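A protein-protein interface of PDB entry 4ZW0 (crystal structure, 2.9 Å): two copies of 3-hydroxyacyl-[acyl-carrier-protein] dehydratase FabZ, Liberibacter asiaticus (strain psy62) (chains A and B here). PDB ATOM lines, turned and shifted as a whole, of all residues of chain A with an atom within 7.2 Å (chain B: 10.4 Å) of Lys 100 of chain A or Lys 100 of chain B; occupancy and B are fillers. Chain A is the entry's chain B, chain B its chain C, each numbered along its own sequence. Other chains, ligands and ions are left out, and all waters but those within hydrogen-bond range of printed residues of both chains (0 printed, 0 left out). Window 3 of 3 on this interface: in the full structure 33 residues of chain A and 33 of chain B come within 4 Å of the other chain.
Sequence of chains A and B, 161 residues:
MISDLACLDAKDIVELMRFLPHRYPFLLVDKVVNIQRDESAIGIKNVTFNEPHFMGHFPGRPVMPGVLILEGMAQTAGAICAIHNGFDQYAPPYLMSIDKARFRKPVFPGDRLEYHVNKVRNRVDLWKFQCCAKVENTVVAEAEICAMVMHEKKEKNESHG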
ATOM      1  N   SER A  97     -20.095  11.557  15.507  1.00  0.00           N
ATOM      2  CA  SER A  97     -21.155  12.473  16.005  1.00  0.00           C
ATOM      3  C   SER A  97     -21.662  13.509  14.988  1.00  0.00           C
ATOM      4  O   SER A  97     -20.942  13.958  14.079  1.00  0.00           O
ATOM      5  CB  SER A  97     -20.711  13.205  17.285  1.00  0.00           C
ATOM      6  OG  SER A  97     -19.957  14.394  17.006  1.00  0.00           O
ATOM      7  N   ILE A  98     -22.916  13.893  15.155  1.00  0.00           N
ATOM      8  CA  ILE A  98     -23.420  15.088  14.500  1.00  0.00           C
ATOM      9  C   ILE A  98     -24.183  15.871  15.548  1.00  0.00           C
ATOM     10  O   ILE A  98     -25.031  15.311  16.247  1.00  0.00           O
ATOM     11  CB  ILE A  98     -24.339  14.766  13.326  1.00  0.00           C
ATOM     12  CG1 ILE A  98     -23.627  13.828  12.343  1.00  0.00           C
ATOM     13  CG2 ILE A  98     -24.757  16.047  12.619  1.00  0.00           C
ATOM     14  CD1 ILE A  98     -24.482  13.365  11.200  1.00  0.00           C
ATOM     15  N   ASP A  99     -23.866  17.155  15.685  1.00  0.00           N
ATOM     16  CA  ASP A  99     -24.557  17.990  16.664  1.00  0.00           C
ATOM     17  C   ASP A  99     -24.929  19.338  16.115  1.00  0.00           C
ATOM     18  O   ASP A  99     -24.269  19.832  15.207  1.00  0.00           O
ATOM     19  CB  ASP A  99     -23.713  18.164  17.923  1.00  0.00           C
ATOM     20  CG  ASP A  99     -24.323  17.463  19.113  1.00  0.00           C
ATOM     21  OD1 ASP A  99     -23.929  16.291  19.366  1.00  0.00           O
ATOM     22  OD2 ASP A  99     -25.216  18.071  19.768  1.00  0.00           O
ATOM     23  N   LYS A 100     -25.981  19.922  16.681  1.00  0.00           N
ATOM     24  CA  LYS A 100     -26.443  21.260  16.306  1.00  0.00           C
ATOM     25  C   LYS A 100     -26.711  21.304  14.829  1.00  0.00           C
ATOM     26  O   LYS A 100     -26.396  22.287  14.175  1.00  0.00           O
ATOM     27  CB  LYS A 100     -25.409  22.347  16.650  1.00  0.00           C
ATOM     28  CG  LYS A 100     -24.739  22.240  18.031  1.00  0.00           C
ATOM     29  CD  LYS A 100     -25.767  22.245  19.148  1.00  0.00           C
ATOM     30  CE  LYS A 100     -25.165  21.832  20.502  1.00  0.00           C
ATOM     31  NZ  LYS A 100     -26.232  21.637  21.543  1.00  0.00           N
ATOM     32  N   ALA A 101     -27.254  20.223  14.286  1.00  0.00           N
ATOM     33  CA  ALA A 101     -27.567  20.177  12.863  1.00  0.00           C
ATOM     34  C   ALA A 101     -28.907  20.860  12.625  1.00  0.00           C
ATOM     35  O   ALA A 101     -29.914  20.545  13.255  1.00  0.00           O
ATOM     36  CB  ALA A 101     -27.584  18.755  12.361  1.00  0.00           C
ATOM     37  N   ARG A 102     -28.915  21.804  11.698  1.00  0.00           N
ATOM     38  CA  ARG A 102     -30.045  22.700  11.545  1.00  0.00           C
ATOM     39  C   ARG A 102     -30.268  22.979  10.069  1.00  0.00           C
ATOM     40  O   ARG A 102     -29.358  23.402   9.363  1.00  0.00           O
ATOM     41  CB  ARG A 102     -29.723  23.977  12.315  1.00  0.00           C
ATOM     42  CG  ARG A 102     -30.914  24.779  12.721  1.00  0.00           C
ATOM     43  CD  ARG A 102     -30.542  26.228  13.095  1.00  0.00           C
ATOM     44  NE  ARG A 102     -31.731  27.038  13.385  1.00  0.00           N
ATOM     45  CZ  ARG A 102     -32.173  27.359  14.606  1.00  0.00           C
ATOM     46  NH1 ARG A 102     -31.541  26.963  15.706  1.00  0.00           N
ATOM     47  NH2 ARG A 102     -33.263  28.101  14.734  1.00  0.00           N
ATOM     48  N   PHE A 103     -31.481  22.710   9.594  1.00  0.00           N
ATOM     49  CA  PHE A 103     -31.805  22.839   8.168  1.00  0.00           C
ATOM     50  C   PHE A 103     -32.775  23.988   7.978  1.00  0.00           C
ATOM     51  O   PHE A 103     -33.872  23.968   8.516  1.00  0.00           O
ATOM     52  CB  PHE A 103     -32.390  21.537   7.615  1.00  0.00           C
ATOM     53  CG  PHE A 103     -31.478  20.345   7.781  1.00  0.00           C
ATOM     54  CD1 PHE A 103     -30.332  20.191   6.991  1.00  0.00           C
ATOM     55  CD2 PHE A 103     -31.755  19.382   8.737  1.00  0.00           C
ATOM     56  CE1 PHE A 103     -29.494  19.113   7.161  1.00  0.00           C
ATOM     57  CE2 PHE A 103     -30.917  18.302   8.919  1.00  0.00           C
ATOM     58  CZ  PHE A 103     -29.779  18.162   8.124  1.00  0.00           C
ATOM     59  N   GLN A 130     -16.760  22.413  12.109  1.00  0.00           N
ATOM     60  CA  GLN A 130     -17.961  23.241  12.101  1.00  0.00           C
ATOM     61  C   GLN A 130     -18.274  23.557  10.644  1.00  0.00           C
ATOM     62  O   GLN A 130     -17.436  24.086   9.913  1.00  0.00           O
ATOM     63  CB  GLN A 130     -17.750  24.519  12.912  1.00  0.00           C
ATOM     64  CG  GLN A 130     -18.921  25.463  12.809  1.00  0.00           C
ATOM     65  CD  GLN A 130     -20.211  24.859  13.381  1.00  0.00           C
ATOM     66  OE1 GLN A 130     -20.164  24.104  14.367  1.00  0.00           O
ATOM     67  NE2 GLN A 130     -21.368  25.191  12.767  1.00  0.00           N
ATOM     68  N   CYS A 131     -19.470  23.183  10.205  1.00  0.00           N
ATOM     69  CA  CYS A 131     -19.792  23.220   8.785  1.00  0.00           C
ATOM     70  C   CYS A 131     -21.099  23.922   8.588  1.00  0.00           C
ATOM     71  O   CYS A 131     -22.015  23.815   9.405  1.00  0.00           O
ATOM     72  CB  CYS A 131     -19.892  21.815   8.185  1.00  0.00           C
ATOM     73  SG  CYS A 131     -18.818  20.587   8.909  1.00  0.00           S
ATOM     74  N   ALA A 141     -28.026  25.157   5.453  1.00  0.00           N
ATOM     75  CA  ALA A 141     -27.903  24.266   6.627  1.00  0.00           C
ATOM     76  C   ALA A 141     -26.645  24.499   7.460  1.00  0.00           C
ATOM     77  O   ALA A 141     -25.716  25.189   7.065  1.00  0.00           O
ATOM     78  CB  ALA A 141     -28.000  22.791   6.208  1.00  0.00           C
ATOM     79  N   GLU A 142     -26.613  23.912   8.631  1.00  0.00           N
ATOM     80  CA  GLU A 142     -25.379  23.914   9.396  1.00  0.00           C
ATOM     81  C   GLU A 142     -25.291  22.734  10.379  1.00  0.00           C
ATOM     82  O   GLU A 142     -26.293  22.291  10.961  1.00  0.00           O
ATOM     83  CB  GLU A 142     -25.246  25.224  10.152  1.00  0.00           C
ATOM     84  CG  GLU A 142     -26.432  25.471  11.068  1.00  0.00           C
ATOM     85  CD  GLU A 142     -26.438  26.847  11.726  1.00  0.00           C
ATOM     86  OE1 GLU A 142     -26.952  26.958  12.870  1.00  0.00           O
ATOM     87  OE2 GLU A 142     -25.951  27.812  11.090  1.00  0.00           O
ATOM     88  N   ALA A 143     -24.084  22.218  10.576  1.00  0.00           N
ATOM     89  CA  ALA A 143     -23.883  21.233  11.622  1.00  0.00           C
ATOM     90  C   ALA A 143     -22.448  21.259  12.133  1.00  0.00           C
ATOM     91  O   ALA A 143     -21.542  21.834  11.527  1.00  0.00           O
ATOM     92  CB  ALA A 143     -24.284  19.819  11.134  1.00  0.00           C
ATOM     93  N   GLU A 144     -22.274  20.629  13.278  1.00  0.00           N
ATOM     94  CA  GLU A 144     -20.966  20.258  13.767  1.00  0.00           C
ATOM     95  C   GLU A 144     -20.789  18.725  13.639  1.00  0.00           C
ATOM     96  O   GLU A 144     -21.538  17.934  14.233  1.00  0.00           O
ATOM     97  CB  GLU A 144     -20.866  20.705  15.208  1.00  0.00           C
ATOM     98  CG  GLU A 144     -19.603  20.305  15.933  1.00  0.00           C
ATOM     99  CD  GLU A 144     -19.626  20.762  17.383  1.00  0.00           C
ATOM    100  OE1 GLU A 144     -18.641  20.483  18.106  1.00  0.00           O
ATOM    101  OE2 GLU A 144     -20.630  21.399  17.796  1.00  0.00           O
ATOM    102  N   LEU B  70     -29.708   7.611  10.642  1.00  0.00           N
ATOM    103  CA  LEU B  70     -30.463   8.784  11.132  1.00  0.00           C
ATOM    104  C   LEU B  70     -31.754   8.839  10.395  1.00  0.00           C
ATOM    105  O   LEU B  70     -32.812   8.947  11.000  1.00  0.00           O
ATOM    106  CB  LEU B  70     -29.710  10.091  10.884  1.00  0.00           C
ATOM    107  CG  LEU B  70     -28.495  10.284  11.782  1.00  0.00           C
ATOM    108  CD1 LEU B  70     -27.873  11.628  11.514  1.00  0.00           C
ATOM    109  CD2 LEU B  70     -28.927  10.125  13.220  1.00  0.00           C
ATOM    110  N   MET B  73     -34.306   6.136  11.549  1.00  0.00           N
ATOM    111  CA  MET B  73     -34.942   6.704  12.735  1.00  0.00           C
ATOM    112  C   MET B  73     -36.026   7.773  12.450  1.00  0.00           C
ATOM    113  O   MET B  73     -37.160   7.709  12.967  1.00  0.00           O
ATOM    114  CB  MET B  73     -33.868   7.310  13.628  1.00  0.00           C
ATOM    115  CG  MET B  73     -32.859   6.335  14.222  1.00  0.00           C
ATOM    116  SD  MET B  73     -31.641   7.373  15.056  1.00  0.00           S
ATOM    117  CE  MET B  73     -30.383   6.195  15.541  1.00  0.00           C
ATOM    118  N   MET B  96     -35.858  19.194  10.192  1.00  0.00           N
ATOM    119  CA  MET B  96     -35.427  20.510  10.680  1.00  0.00           C
ATOM    120  C   MET B  96     -34.179  20.485  11.566  1.00  0.00           C
ATOM    121  O   MET B  96     -33.314  21.356  11.447  1.00  0.00           O
ATOM    122  CB  MET B  96     -36.577  21.221  11.410  1.00  0.00           C
ATOM    123  CG  MET B  96     -37.721  21.568  10.503  1.00  0.00           C
ATOM    124  SD  MET B  96     -39.003  22.535  11.299  1.00  0.00           S
ATOM    125  CE  MET B  96     -38.484  24.166  10.848  1.00  0.00           C
ATOM    126  N   SER B  97     -34.081  19.510  12.467  1.00  0.00           N
ATOM    127  CA  SER B  97     -32.896  19.465  13.300  1.00  0.00           C
ATOM    128  C   SER B  97     -32.487  18.044  13.616  1.00  0.00           C
ATOM    129  O   SER B  97     -33.326  17.135  13.657  1.00  0.00           O
ATOM    130  CB  SER B  97     -33.119  20.203  14.617  1.00  0.00           C
ATOM    131  OG  SER B  97     -33.707  19.332  15.585  1.00  0.00           O
ATOM    132  N   ILE B  98     -31.185  17.874  13.866  1.00  0.00           N
ATOM    133  CA  ILE B  98     -30.662  16.666  14.476  1.00  0.00           C
ATOM    134  C   ILE B  98     -29.687  17.098  15.538  1.00  0.00           C
ATOM    135  O   ILE B  98     -28.778  17.874  15.266  1.00  0.00           O
ATOM    136  CB  ILE B  98     -29.968  15.743  13.424  1.00  0.00           C
ATOM    137  CG1 ILE B  98     -30.899  15.452  12.251  1.00  0.00           C
ATOM    138  CG2 ILE B  98     -29.559  14.403  14.010  1.00  0.00           C
ATOM    139  CD1 ILE B  98     -30.199  14.697  11.179  1.00  0.00           C
ATOM    140  N   ASP B  99     -29.879  16.592  16.748  1.00  0.00           N
ATOM    141  CA  ASP B  99     -28.960  16.888  17.836  1.00  0.00           C
ATOM    142  C   ASP B  99     -28.578  15.674  18.647  1.00  0.00           C
ATOM    143  O   ASP B  99     -29.357  14.730  18.752  1.00  0.00           O
ATOM    144  CB  ASP B  99     -29.561  17.935  18.752  1.00  0.00           C
ATOM    145  CG  ASP B  99     -28.855  19.270  18.629  1.00  0.00           C
ATOM    146  OD1 ASP B  99     -29.347  20.141  17.860  1.00  0.00           O
ATOM    147  OD2 ASP B  99     -27.790  19.425  19.288  1.00  0.00           O
ATOM    148  N   LYS B 100     -27.377  15.734  19.233  1.00  0.00           N
ATOM    149  CA  LYS B 100     -26.855  14.685  20.119  1.00  0.00           C
ATOM    150  C   LYS B 100     -26.832  13.378  19.351  1.00  0.00           C
ATOM    151  O   LYS B 100     -27.157  12.323  19.906  1.00  0.00           O
ATOM    152  CB  LYS B 100     -27.694  14.503  21.413  1.00  0.00           C
ATOM    153  CG  LYS B 100     -28.117  15.780  22.161  1.00  0.00           C
ATOM    154  CD  LYS B 100     -26.912  16.626  22.530  1.00  0.00           C
ATOM    155  CE  LYS B 100     -27.290  18.052  22.937  1.00  0.00           C
ATOM    156  NZ  LYS B 100     -26.067  18.940  23.093  1.00  0.00           N
ATOM    157  N   ALA B 101     -26.476  13.450  18.070  1.00  0.00           N
ATOM    158  CA  ALA B 101     -26.339  12.243  17.261  1.00  0.00           C
ATOM    159  C   ALA B 101     -24.967  11.595  17.516  1.00  0.00           C
ATOM    160  O   ALA B 101     -23.877  12.195  17.357  1.00  0.00           O
ATOM    161  CB  ALA B 101     -26.572  12.528  15.783  1.00  0.00           C
ATOM    162  N   ARG B 102     -25.038  10.340  17.933  1.00  0.00           N
ATOM    163  CA  ARG B 102     -23.850   9.624  18.362  1.00  0.00           C
ATOM    164  C   ARG B 102     -23.831   8.204  17.760  1.00  0.00           C
ATOM    165  O   ARG B 102     -24.781   7.405  17.925  1.00  0.00           O
ATOM    166  CB  ARG B 102     -23.848   9.599  19.896  1.00  0.00           C
ATOM    167  CG  ARG B 102     -22.490   9.397  20.545  1.00  0.00           C
ATOM    168  CD  ARG B 102     -22.643   8.941  22.015  1.00  0.00           C
ATOM    169  NE  ARG B 102     -21.352   8.659  22.657  1.00  0.00           N
ATOM    170  CZ  ARG B 102     -20.694   9.500  23.465  1.00  0.00           C
ATOM    171  NH1 ARG B 102     -21.191  10.700  23.770  1.00  0.00           N
ATOM    172  NH2 ARG B 102     -19.527   9.138  23.982  1.00  0.00           N
ATOM    173  N   PHE B 103     -22.755   7.902  17.045  1.00  0.00           N
ATOM    174  CA  PHE B 103     -22.592   6.581  16.438  1.00  0.00           C
ATOM    175  C   PHE B 103     -21.523   5.763  17.179  1.00  0.00           C
ATOM    176  O   PHE B 103     -20.324   6.125  17.198  1.00  0.00           O
ATOM    177  CB  PHE B 103     -22.227   6.733  14.944  1.00  0.00           C
ATOM    178  CG  PHE B 103     -23.220   7.569  14.159  1.00  0.00           C
ATOM    179  CD1 PHE B 103     -24.508   7.097  13.889  1.00  0.00           C
ATOM    180  CD2 PHE B 103     -22.874   8.827  13.707  1.00  0.00           C
ATOM    181  CE1 PHE B 103     -25.420   7.872  13.175  1.00  0.00           C
ATOM    182  CE2 PHE B 103     -23.785   9.603  13.002  1.00  0.00           C
ATOM    183  CZ  PHE B 103     -25.057   9.124  12.733  1.00  0.00           C
ATOM    184  N   ARG B 104     -21.951   4.645  17.758  1.00  0.00           N
ATOM    185  CA  ARG B 104     -21.076   3.847  18.621  1.00  0.00           C
ATOM    186  C   ARG B 104     -20.445   2.644  17.986  1.00  0.00           C
ATOM    187  O   ARG B 104     -19.378   2.209  18.386  1.00  0.00           O
ATOM    188  CB  ARG B 104     -21.881   3.376  19.806  1.00  0.00           C
ATOM    189  CG  ARG B 104     -22.525   4.537  20.486  1.00  0.00           C
ATOM    190  CD  ARG B 104     -23.284   4.060  21.650  1.00  0.00           C
ATOM    191  NE  ARG B 104     -23.703   5.155  22.517  1.00  0.00           N
ATOM    192  CZ  ARG B 104     -24.263   4.958  23.707  1.00  0.00           C
ATOM    193  NH1 ARG B 104     -24.450   3.713  24.156  1.00  0.00           N
ATOM    194  NH2 ARG B 104     -24.630   5.993  24.447  1.00  0.00           N
ATOM    195  N   LYS B 128     -40.641  16.085  17.597  1.00  0.00           N
ATOM    196  CA  LYS B 128     -39.253  15.946  17.963  1.00  0.00           C
ATOM    197  C   LYS B 128     -39.177  14.691  18.783  1.00  0.00           C
ATOM    198  O   LYS B 128     -39.759  14.663  19.855  1.00  0.00           O
ATOM    199  CB  LYS B 128     -38.806  17.120  18.828  1.00  0.00           C
ATOM    200  CG  LYS B 128     -37.515  16.875  19.577  1.00  0.00           C
ATOM    201  CD  LYS B 128     -37.202  18.001  20.542  1.00  0.00           C
ATOM    202  CE  LYS B 128     -37.071  19.332  19.805  1.00  0.00           C
ATOM    203  NZ  LYS B 128     -36.850  20.491  20.729  1.00  0.00           N
ATOM    204  N   PHE B 129     -38.466  13.662  18.296  1.00  0.00           N
ATOM    205  CA  PHE B 129     -38.299  12.376  19.009  1.00  0.00           C
ATOM    206  C   PHE B 129     -36.893  12.069  19.493  1.00  0.00           C
ATOM    207  O   PHE B 129     -35.882  12.546  18.935  1.00  0.00           O
ATOM    208  CB  PHE B 129     -38.736  11.221  18.145  1.00  0.00           C
ATOM    209  CG  PHE B 129     -40.206  11.058  18.051  1.00  0.00           C
ATOM    210  CD1 PHE B 129     -40.808   9.899  18.506  1.00  0.00           C
ATOM    211  CD2 PHE B 129     -41.002  12.052  17.521  1.00  0.00           C
ATOM    212  CE1 PHE B 129     -42.189   9.713  18.439  1.00  0.00           C
ATOM    213  CE2 PHE B 129     -42.387  11.878  17.442  1.00  0.00           C
ATOM    214  CZ  PHE B 129     -42.977  10.695  17.908  1.00  0.00           C
ATOM    215  N   GLN B 130     -36.846  11.243  20.538  1.00  0.00           N
ATOM    216  CA  GLN B 130     -35.593  10.699  21.040  1.00  0.00           C
ATOM    217  C   GLN B 130     -35.461   9.280  20.517  1.00  0.00           C
ATOM    218  O   GLN B 130     -36.338   8.443  20.730  1.00  0.00           O
ATOM    219  CB  GLN B 130     -35.542  10.703  22.556  1.00  0.00           C
ATOM    220  CG  GLN B 130     -34.250  10.092  23.070  1.00  0.00           C
ATOM    221  CD  GLN B 130     -33.004  10.804  22.538  1.00  0.00           C
ATOM    222  OE1 GLN B 130     -32.980  12.037  22.422  1.00  0.00           O
ATOM    223  NE2 GLN B 130     -31.960  10.028  22.220  1.00  0.00           N
ATOM    224  N   CYS B 131     -34.373   9.022  19.804  1.00  0.00           N
ATOM    225  CA  CYS B 131     -34.250   7.790  19.038  1.00  0.00           C
ATOM    226  C   CYS B 131     -32.934   7.142  19.298  1.00  0.00           C
ATOM    227  O   CYS B 131     -31.867   7.782  19.377  1.00  0.00           O
ATOM    228  CB  CYS B 131     -34.332   8.045  17.536  1.00  0.00           C
ATOM    229  SG  CYS B 131     -35.540   9.299  17.070  1.00  0.00           S
ATOM    230  N   CYS B 132     -33.021   5.834  19.422  1.00  0.00           N
ATOM    231  CA  CYS B 132     -31.835   5.040  19.614  1.00  0.00           C
ATOM    232  C   CYS B 132     -31.928   3.800  18.704  1.00  0.00           C
ATOM    233  O   CYS B 132     -32.984   3.146  18.632  1.00  0.00           O
ATOM    234  CB  CYS B 132     -31.681   4.710  21.106  1.00  0.00           C
ATOM    235  SG  CYS B 132     -31.620   2.981  21.555  1.00  0.00           S
ATOM    236  N   ALA B 133     -30.834   3.526  17.979  1.00  0.00           N
ATOM    237  CA  ALA B 133     -30.719   2.362  17.126  1.00  0.00           C
ATOM    238  C   ALA B 133     -29.912   1.244  17.781  1.00  0.00           C
ATOM    239  O   ALA B 133     -28.737   1.427  18.176  1.00  0.00           O
ATOM    240  CB  ALA B 133     -30.103   2.742  15.837  1.00  0.00           C
ATOM    241  N   VAL B 139     -26.702  -0.959  21.727  1.00  0.00           N
ATOM    242  CA  VAL B 139     -26.963   0.348  21.150  1.00  0.00           C
ATOM    243  C   VAL B 139     -25.867   0.711  20.168  1.00  0.00           C
ATOM    244  O   VAL B 139     -24.688   0.731  20.486  1.00  0.00           O
ATOM    245  CB  VAL B 139     -27.188   1.419  22.218  1.00  0.00           C
ATOM    246  CG1 VAL B 139     -27.157   2.830  21.578  1.00  0.00           C
ATOM    247  CG2 VAL B 139     -28.509   1.129  22.875  1.00  0.00           C
ATOM    248  N   VAL B 140     -26.289   0.997  18.954  1.00  0.00           N
ATOM    249  CA  VAL B 140     -25.356   1.185  17.867  1.00  0.00           C
ATOM    250  C   VAL B 140     -25.317   2.672  17.508  1.00  0.00           C
ATOM    251  O   VAL B 140     -24.261   3.217  17.155  1.00  0.00           O
ATOM    252  CB  VAL B 140     -25.750   0.226  16.731  1.00  0.00           C
ATOM    253  CG1 VAL B 140     -25.496   0.832  15.362  1.00  0.00           C
ATOM    254  CG2 VAL B 140     -25.055  -1.143  16.954  1.00  0.00           C
ATOM    255  N   ALA B 141     -26.465   3.334  17.663  1.00  0.00           N
ATOM    256  CA  ALA B 141     -26.501   4.801  17.492  1.00  0.00           C
ATOM    257  C   ALA B 141     -27.593   5.470  18.308  1.00  0.00           C
ATOM    258  O   ALA B 141     -28.467   4.813  18.873  1.00  0.00           O
ATOM    259  CB  ALA B 141     -26.603   5.225  15.983  1.00  0.00           C
ATOM    260  N   GLU B 142     -27.526   6.789  18.395  1.00  0.00           N
ATOM    261  CA  GLU B 142     -28.622   7.572  19.015  1.00  0.00           C
ATOM    262  C   GLU B 142     -28.646   9.020  18.495  1.00  0.00           C
ATOM    263  O   GLU B 142     -27.597   9.635  18.162  1.00  0.00           O
ATOM    264  CB  GLU B 142     -28.517   7.564  20.539  1.00  0.00           C
ATOM    265  CG  GLU B 142     -27.135   8.024  21.016  1.00  0.00           C
ATOM    266  CD  GLU B 142     -26.902   7.843  22.506  1.00  0.00           C
ATOM    267  OE1 GLU B 142     -26.184   8.688  23.094  1.00  0.00           O
ATOM    268  OE2 GLU B 142     -27.412   6.854  23.078  1.00  0.00           O
ATOM    269  N   ALA B 143     -29.852   9.562  18.407  1.00  0.00           N
ATOM    270  CA  ALA B 143     -30.009  10.973  18.071  1.00  0.00           C
ATOM    271  C   ALA B 143     -31.348  11.512  18.521  1.00  0.00           C
ATOM    272  O   ALA B 143     -32.297  10.770  18.761  1.00  0.00           O
ATOM    273  CB  ALA B 143     -29.816  11.199  16.589  1.00  0.00           C
ATOM    274  N   GLU B 144     -31.410  12.823  18.646  1.00  0.00           N
ATOM    275  CA  GLU B 144     -32.664  13.510  18.853  1.00  0.00           C
ATOM    276  C   GLU B 144     -32.988  14.191  17.533  1.00  0.00           C
ATOM    277  O   GLU B 144     -32.184  14.955  16.989  1.00  0.00           O
ATOM    278  CB  GLU B 144     -32.489  14.516  19.966  1.00  0.00           C
ATOM    279  CG  GLU B 144     -33.716  15.351  20.295  1.00  0.00           C
ATOM    280  CD  GLU B 144     -33.427  16.369  21.394  1.00  0.00           C
ATOM    281  OE1 GLU B 144     -34.330  17.157  21.733  1.00  0.00           O
ATOM    282  OE2 GLU B 144     -32.291  16.383  21.923  1.00  0.00           O
ATOM    283  N   ILE B 145     -34.156  13.872  16.991  1.00  0.00           N
ATOM    284  CA  ILE B 145     -34.490  14.298  15.637  1.00  0.00           C
ATOM    285  C   ILE B 145     -35.768  15.080  15.651  1.00  0.00           C
ATOM    286  O   ILE B 145     -36.787  14.594  16.129  1.00  0.00           O
ATOM    287  CB  ILE B 145     -34.802  13.121  14.668  1.00  0.00           C
ATOM    288  CG1 ILE B 145     -33.894  11.896  14.869  1.00  0.00           C
ATOM    289  CG2 ILE B 145     -34.752  13.592  13.249  1.00  0.00           C
ATOM    290  CD1 ILE B 145     -32.558  12.038  14.301  1.00  0.00           C
ATOM    291  N   CYS B 146     -35.729  16.278  15.085  1.00  0.00           N
ATOM    292  CA  CYS B 146     -36.947  17.063  14.896  1.00  0.00           C
ATOM    293  C   CYS B 146     -37.332  17.363  13.419  1.00  0.00           C
ATOM    294  O   CYS B 146     -36.510  17.808  12.609  1.00  0.00           O
ATOM    295  CB  CYS B 146     -36.868  18.355  15.715  1.00  0.00           C
ATOM    296  SG  CYS B 146     -38.237  19.455  15.290  1.00  0.00           S
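N of Ile 98 of chain A is in hydrogen-bond range of O of Ala 101 of chain B. The side-chain carboxylate (OD2) of Asp 99 of chain A is in salt-bridge range of the side-chain amino group (NZ) of Lys 100 of chain B (3.5 Å). NZ of Lys 100 of chain A lies within salt-bridge range of OD2 of Asp 99 of chain B (3.5 Å). The backbone NH (N) of Ala 101 of chain A is in hydrogen-bond range of the backbone carbonyl oxygen (O) of Ile 98 of chain B, 3.0 Å away. The backbone carbonyl oxygen of Met 96 of chain B is in hydrogen-bond range of the backbone NH of Phe 103 of chain A (2.9 Å). OD2 of Asp 99 of chain A lies close to OD2 of Asp 99 of chain B, 2.9 Å away. The side-chain amino group of Lys 100 of chain A lies close to the side-chain amino group of Lys 100 of chain B (3.1 Å).
Lys 100 of chain A touches just these residues of chain B: Ile 98 (3.7 Å), Asp 99 (3.2 Å) and Lys 100 (3.1 Å). Of chain A, only Ile 98, Asp 99 and Lys 100 come within 4 Å of Lys 100 of chain B. Of chain B, only Met 96, Ser 97 and Ile 98 come within 4 Å of Ala 101 of chain A. No residue of chain B comes within 4 Å of Glu 142 of chain A. No residue of chain B comes within 4 Å of Ala 143 of chain A. Printed residues of chain A within 4 Å of Ala 101 of chain B: Ser 97 (3.1 Å) and Ile 98 (2.9 Å). Of the printed residues of chain B, Ser 97 of chain A touches Ala 101. Printed residues of chain B within 4 Å of Phe 103 of chain A: Met 96 (2.9 Å). Cys 131 of chain B touches none of the printed residues of chain A. Ile 145 of chain B touches none of the printed residues of chain A. The nearest residue of chain A that does not touch Lys 100 of chain B is Ser 97 of chain A (6.5 Å). The nearest printed residue of chain B that does not touch Ile 98 of chain A is Phe 103 of chain B (4.2 Å).
Among the printed residues, merely in contact across the chains: Ser 97 of chain A with Ala 101 of chain B (3.1 Å), Ile 98 of chain A with Leu 70 of chain B (3.8 Å), Ile 98 of chain A with Lys 100 of chain B (3.8 Å), Lys 100 of chain A with Ile 98 of chain B (3.7 Å), Ala 101 of chain A with Met 96 of chain B (3.9 Å), Ala 101 of chain A with Ser 97 of chain B (3.2 Å) and Arg 102 of chain A with Met 96 of chain B (3.5 Å).
Ser 97 of chain A touches Ala 101 of chain B, and with the chains exchanged Ala 101 of chain A touches Ser 97 of chain B. Asp 99 of chain A touches Lys 100 of chain B, and with the chains exchanged Lys 100 of chain A touches Asp 99 of chain B. Lys 100 of chain A touches its own counterpart, Lys 100 of chain B. Of the 14 pairs that touch across the chains among the printed residues, 10 have their exchanged pair printed and touching as well.
Printed residues of chain A that touch a printed residue of chain B: Ser 97, Ile 98, Asp 99, Lys 100, Ala 101, Arg 102 and Phe 103. Along chain A the printed residues that touch a printed residue of chain B span positions 97 to 103. Among the printed residues, 14 pairs touch across the chains. Among the printed residues, Asp or Glu carboxylates within 4 Å of a Lys or Arg side-chain nitrogen of the other chain: Asp 99 of chain A with Lys 100 of chain B (3.5 Å) and Lys 100 of chain A with Asp 99 of chain B (3.5 Å).
The backbone NH (N) of Met 96 of chain B lies within hydrogen-bond range of the backbone carbonyl oxygen (O) of Cys 146 of chain B (2.9 Å). The backbone carbonyl oxygen (O) of Ser 97 of chain B is in hydrogen-bond range of the backbone NH (N) of Cys 146 of chain B, at 2.9 Å. The backbone carbonyl oxygen (O) of Asp 99 of chain B lies within hydrogen-bond range of the backbone NH (N) of Glu 144 of chain B (2.8 Å).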
